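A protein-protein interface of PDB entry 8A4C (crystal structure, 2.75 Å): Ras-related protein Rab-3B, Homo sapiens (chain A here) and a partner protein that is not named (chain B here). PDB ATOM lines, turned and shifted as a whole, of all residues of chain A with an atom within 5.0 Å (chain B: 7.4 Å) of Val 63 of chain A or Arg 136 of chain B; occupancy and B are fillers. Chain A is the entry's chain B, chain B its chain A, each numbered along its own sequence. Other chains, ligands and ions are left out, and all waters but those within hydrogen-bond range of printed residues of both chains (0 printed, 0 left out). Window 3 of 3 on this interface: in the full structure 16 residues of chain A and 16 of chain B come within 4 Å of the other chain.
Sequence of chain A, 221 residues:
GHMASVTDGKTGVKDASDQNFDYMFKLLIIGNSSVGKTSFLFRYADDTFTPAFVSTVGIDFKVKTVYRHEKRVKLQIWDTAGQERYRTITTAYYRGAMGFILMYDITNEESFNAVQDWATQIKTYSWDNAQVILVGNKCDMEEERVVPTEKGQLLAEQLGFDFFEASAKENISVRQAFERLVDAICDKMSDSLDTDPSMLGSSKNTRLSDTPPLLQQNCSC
CD2 of His 86 of chain B touches O of Phe 61 of chain A, 3.2 Å away. CE2 of Phe 61 of chain A touches CB of Arg 136 of chain B, at 3.9 Å. Phe 61 of chain A touches Val 137 of chain B (CZ to CG1, 3.6 Å). Arg 136 of chain B touches Lys 62 of chain A (NH2 to NZ, 3.97 Å). Val 137 of chain B touches Gln 76 of chain A (CG1 to OE1, 3.6 Å).
Printed residues of chain A that touch a printed residue of chain B: Phe 61, Lys 62, Val 63 and Gln 76. Hydrophobic or aromatic side chains of chain B within 4 Å of the printed part of chain A: His 86 and Val 137. Among the printed residues, 6 pairs touch across the chains. Among the printed residues, no Asp or Glu carboxylate lies within 4 Å of a Lys or Arg side-chain nitrogen of the other chain.
Val 63 of chain A touches one residue of chain B. Of the printed residues of chain A, Val 137 of chain B touches Phe 61 and Gln 76. Of the printed residues of chain A, His 86 of chain B touches Phe 61. Printed residues of chain B within 4 Å of Lys 62 of chain A: Arg 136. The nearest residue of chain B that does not touch Val 63 of chain A is Val 137 of chain B (5.6 Å). The nearest printed residue of chain A that does not touch Arg 136 of chain B is Gln 76 of chain A (5.0 Å). The nearest printed residue of chain B that does not touch Lys 62 of chain A is His 86 of chain B (5.2 Å).
The guanidinium group (NH1) of Arg 136 of chain B is in hydrogen-bond range of the backbone carbonyl oxygen (O) of Val 63 of chain A (3.1 Å).
A ring nitrogen (NE2) of His 86 of chain B lies within hydrogen-bond range of the guanidinium group (NE) of Arg 136 of chain B, at 3.0 Å.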
ATOM      1  N   PHE A  61     -33.108  22.430  28.812  1.00  0.00           N
ATOM      2  CA  PHE A  61     -33.416  23.800  28.421  1.00  0.00           C
ATOM      3  C   PHE A  61     -33.337  23.950  26.906  1.00  0.00           C
ATOM      4  O   PHE A  61     -32.671  23.179  26.211  1.00  0.00           O
ATOM      5  CB  PHE A  61     -32.487  24.816  29.116  1.00  0.00           C
ATOM      6  CG  PHE A  61     -31.073  24.821  28.594  1.00  0.00           C
ATOM      7  CD1 PHE A  61     -30.152  23.899  29.064  1.00  0.00           C
ATOM      8  CD2 PHE A  61     -30.653  25.771  27.660  1.00  0.00           C
ATOM      9  CE1 PHE A  61     -28.851  23.904  28.601  1.00  0.00           C
ATOM     10  CE2 PHE A  61     -29.356  25.773  27.185  1.00  0.00           C
ATOM     11  CZ  PHE A  61     -28.456  24.836  27.655  1.00  0.00           C
ATOM     12  N   LYS A  62     -34.023  24.977  26.409  1.00  0.00           N
ATOM     13  CA  LYS A  62     -33.984  25.372  25.006  1.00  0.00           C
ATOM     14  C   LYS A  62     -33.830  26.886  24.925  1.00  0.00           C
ATOM     15  O   LYS A  62     -34.209  27.615  25.843  1.00  0.00           O
ATOM     16  CB  LYS A  62     -35.247  24.932  24.246  1.00  0.00           C
ATOM     17  CG  LYS A  62     -35.423  23.426  24.123  1.00  0.00           C
ATOM     18  CD  LYS A  62     -36.251  23.056  22.902  1.00  0.00           C
ATOM     19  CE  LYS A  62     -35.778  21.746  22.287  1.00  0.00           C
ATOM     20  NZ  LYS A  62     -35.271  21.944  20.898  1.00  0.00           N
ATOM     21  N   VAL A  63     -33.271  27.362  23.822  1.00  0.00           N
ATOM     22  CA  VAL A  63     -33.058  28.789  23.614  1.00  0.00           C
ATOM     23  C   VAL A  63     -33.909  29.232  22.436  1.00  0.00           C
ATOM     24  O   VAL A  63     -33.859  28.625  21.359  1.00  0.00           O
ATOM     25  CB  VAL A  63     -31.571  29.114  23.392  1.00  0.00           C
ATOM     26  CG1 VAL A  63     -31.389  30.520  22.828  1.00  0.00           C
ATOM     27  CG2 VAL A  63     -30.802  28.947  24.693  1.00  0.00           C
ATOM     28  N   LYS A  64     -34.713  30.270  22.652  1.00  0.00           N
ATOM     29  CA  LYS A  64     -35.527  30.858  21.603  1.00  0.00           C
ATOM     30  C   LYS A  64     -35.274  32.356  21.575  1.00  0.00           C
ATOM     31  O   LYS A  64     -35.263  33.002  22.625  1.00  0.00           O
ATOM     32  CB  LYS A  64     -37.017  30.568  21.827  1.00  0.00           C
ATOM     33  CG  LYS A  64     -37.921  31.030  20.684  1.00  0.00           C
ATOM     34  CD  LYS A  64     -39.328  30.492  20.847  1.00  0.00           C
ATOM     35  CE  LYS A  64     -40.274  31.033  19.792  1.00  0.00           C
ATOM     36  NZ  LYS A  64     -39.870  30.616  18.426  1.00  0.00           N
ATOM     37  N   THR A  65     -35.066  32.905  20.381  1.00  0.00           N
ATOM     38  CA  THR A  65     -34.937  34.344  20.194  1.00  0.00           C
ATOM     39  C   THR A  65     -36.254  34.908  19.682  1.00  0.00           C
ATOM     40  O   THR A  65     -36.897  34.315  18.810  1.00  0.00           O
ATOM     41  CB  THR A  65     -33.801  34.674  19.223  1.00  0.00           C
ATOM     42  OG1 THR A  65     -32.720  33.751  19.414  1.00  0.00           O
ATOM     43  CG2 THR A  65     -33.298  36.089  19.446  1.00  0.00           C
ATOM     44  N   LYS A  74     -33.278  37.044  23.881  1.00  0.00           N
ATOM     45  CA  LYS A  74     -32.926  35.627  23.924  1.00  0.00           C
ATOM     46  C   LYS A  74     -33.403  35.002  25.233  1.00  0.00           C
ATOM     47  O   LYS A  74     -32.917  35.350  26.312  1.00  0.00           O
ATOM     48  CB  LYS A  74     -31.416  35.420  23.714  1.00  0.00           C
ATOM     49  CG  LYS A  74     -31.025  35.001  22.250  1.00  0.00           C
ATOM     50  CD  LYS A  74     -29.504  34.917  21.966  1.00  0.00           C
ATOM     51  CE  LYS A  74     -29.120  35.185  20.499  1.00  0.00           C
ATOM     52  NZ  LYS A  74     -29.185  36.572  19.947  1.00  0.00           N
ATOM     53  N   LEU A  75     -34.355  34.076  25.129  1.00  0.00           N
ATOM     54  CA  LEU A  75     -34.887  33.341  26.270  1.00  0.00           C
ATOM     55  C   LEU A  75     -34.220  31.978  26.364  1.00  0.00           C
ATOM     56  O   LEU A  75     -34.298  31.180  25.422  1.00  0.00           O
ATOM     57  CB  LEU A  75     -36.398  33.148  26.153  1.00  0.00           C
ATOM     58  CG  LEU A  75     -37.298  34.276  25.679  1.00  0.00           C
ATOM     59  CD1 LEU A  75     -38.744  33.786  25.586  1.00  0.00           C
ATOM     60  CD2 LEU A  75     -37.180  35.403  26.675  1.00  0.00           C
ATOM     61  N   GLN A  76     -33.601  31.695  27.504  1.00  0.00           N
ATOM     62  CA  GLN A  76     -33.255  30.322  27.827  1.00  0.00           C
ATOM     63  C   GLN A  76     -34.317  29.784  28.786  1.00  0.00           C
ATOM     64  O   GLN A  76     -34.524  30.319  29.884  1.00  0.00           O
ATOM     65  CB  GLN A  76     -31.815  30.189  28.345  1.00  0.00           C
ATOM     66  CG  GLN A  76     -31.413  30.795  29.681  1.00  0.00           C
ATOM     67  CD  GLN A  76     -30.110  30.191  30.189  1.00  0.00           C
ATOM     68  OE1 GLN A  76     -29.412  29.492  29.450  1.00  0.00           O
ATOM     69  NE2 GLN A  76     -29.787  30.443  31.454  1.00  0.00           N
ATOM     70  N   LYS B  85     -27.433  16.697  24.445  1.00  0.00           N
ATOM     71  CA  LYS B  85     -26.155  17.404  24.427  1.00  0.00           C
ATOM     72  C   LYS B  85     -26.077  18.414  25.565  1.00  0.00           C
ATOM     73  O   LYS B  85     -25.050  18.516  26.250  1.00  0.00           O
ATOM     74  CB  LYS B  85     -25.941  18.102  23.069  1.00  0.00           C
ATOM     75  CG  LYS B  85     -26.270  17.305  21.765  1.00  0.00           C
ATOM     76  CD  LYS B  85     -27.766  17.317  21.338  1.00  0.00           C
ATOM     77  CE  LYS B  85     -27.974  17.112  19.850  1.00  0.00           C
ATOM     78  NZ  LYS B  85     -29.303  17.655  19.440  1.00  0.00           N
ATOM     79  N   HIS B  86     -27.178  19.131  25.807  1.00  0.00           N
ATOM     80  CA  HIS B  86     -27.279  20.013  26.964  1.00  0.00           C
ATOM     81  C   HIS B  86     -27.192  19.229  28.265  1.00  0.00           C
ATOM     82  O   HIS B  86     -26.474  19.623  29.189  1.00  0.00           O
ATOM     83  CB  HIS B  86     -28.594  20.786  26.914  1.00  0.00           C
ATOM     84  CG  HIS B  86     -28.733  21.679  25.723  1.00  0.00           C
ATOM     85  ND1 HIS B  86     -27.648  22.200  25.051  1.00  0.00           N
ATOM     86  CD2 HIS B  86     -29.831  22.152  25.088  1.00  0.00           C
ATOM     87  CE1 HIS B  86     -28.071  22.950  24.051  1.00  0.00           C
ATOM     88  NE2 HIS B  86     -29.392  22.938  24.052  1.00  0.00           N
ATOM     89  N   PRO B 133     -17.769  22.509  25.097  1.00  0.00           N
ATOM     90  CA  PRO B 133     -18.879  22.208  24.188  1.00  0.00           C
ATOM     91  C   PRO B 133     -20.245  22.522  24.799  1.00  0.00           C
ATOM     92  O   PRO B 133     -21.138  21.671  24.790  1.00  0.00           O
ATOM     93  CB  PRO B 133     -18.721  20.707  23.936  1.00  0.00           C
ATOM     94  CG  PRO B 133     -17.261  20.467  24.085  1.00  0.00           C
ATOM     95  CD  PRO B 133     -16.809  21.392  25.182  1.00  0.00           C
ATOM     96  N   GLU B 134     -20.396  23.740  25.323  1.00  0.00           N
ATOM     97  CA  GLU B 134     -21.658  24.154  25.930  1.00  0.00           C
ATOM     98  C   GLU B 134     -22.719  24.457  24.873  1.00  0.00           C
ATOM     99  O   GLU B 134     -23.860  23.988  24.980  1.00  0.00           O
ATOM    100  CB  GLU B 134     -21.420  25.362  26.845  1.00  0.00           C
ATOM    101  CG  GLU B 134     -20.461  26.433  26.313  1.00  0.00           C
ATOM    102  CD  GLU B 134     -20.256  27.579  27.288  1.00  0.00           C
ATOM    103  OE1 GLU B 134     -20.032  27.315  28.487  1.00  0.00           O
ATOM    104  OE2 GLU B 134     -20.335  28.748  26.854  1.00  0.00           O
ATOM    105  N   SER B 135     -22.364  25.299  23.896  1.00  0.00           N
ATOM    106  CA  SER B 135     -23.020  25.574  22.617  1.00  0.00           C
ATOM    107  C   SER B 135     -24.323  26.371  22.691  1.00  0.00           C
ATOM    108  O   SER B 135     -24.768  26.882  21.658  1.00  0.00           O
ATOM    109  CB  SER B 135     -23.277  24.264  21.853  1.00  0.00           C
ATOM    110  OG  SER B 135     -24.624  23.835  21.991  1.00  0.00           O
ATOM    111  N   ARG B 136     -24.926  26.539  23.876  1.00  0.00           N
ATOM    112  CA  ARG B 136     -26.098  27.417  23.977  1.00  0.00           C
ATOM    113  C   ARG B 136     -26.156  28.306  25.218  1.00  0.00           C
ATOM    114  O   ARG B 136     -26.831  29.339  25.162  1.00  0.00           O
ATOM    115  CB  ARG B 136     -27.407  26.610  23.888  1.00  0.00           C
ATOM    116  CG  ARG B 136     -27.854  26.289  22.447  1.00  0.00           C
ATOM    117  CD  ARG B 136     -29.360  26.444  22.220  1.00  0.00           C
ATOM    118  NE  ARG B 136     -30.074  25.172  22.162  1.00  0.00           N
ATOM    119  CZ  ARG B 136     -31.333  25.025  21.767  1.00  0.00           C
ATOM    120  NH1 ARG B 136     -32.057  26.054  21.367  1.00  0.00           N
ATOM    121  NH2 ARG B 136     -31.875  23.810  21.765  1.00  0.00           N
ATOM    122  N   VAL B 137     -25.499  27.971  26.332  1.00  0.00           N
ATOM    123  CA  VAL B 137     -25.614  28.788  27.541  1.00  0.00           C
ATOM    124  C   VAL B 137     -24.708  30.008  27.450  1.00  0.00           C
ATOM    125  O   VAL B 137     -23.810  30.076  26.602  1.00  0.00           O
ATOM    126  CB  VAL B 137     -25.304  27.986  28.822  1.00  0.00           C
ATOM    127  CG1 VAL B 137     -26.556  27.335  29.369  1.00  0.00           C
ATOM    128  CG2 VAL B 137     -24.249  26.943  28.559  1.00  0.00           C
ATOM    129  N   GLU B 138     -24.938  30.976  28.332  1.00  0.00           N
ATOM    130  CA  GLU B 138     -24.140  32.194  28.377  1.00  0.00           C
ATOM    131  C   GLU B 138     -22.828  31.956  29.118  1.00  0.00           C
ATOM    132  O   GLU B 138     -21.780  32.468  28.725  1.00  0.00           O
ATOM    133  CB  GLU B 138     -24.930  33.321  29.046  1.00  0.00           C
ATOM    134  CG  GLU B 138     -24.296  34.694  28.918  1.00  0.00           C
ATOM    135  CD  GLU B 138     -24.972  35.729  29.794  1.00  0.00           C
ATOM    136  OE1 GLU B 138     -25.546  35.342  30.835  1.00  0.00           O
ATOM    137  OE2 GLU B 138     -24.928  36.927  29.444  1.00  0.00           O
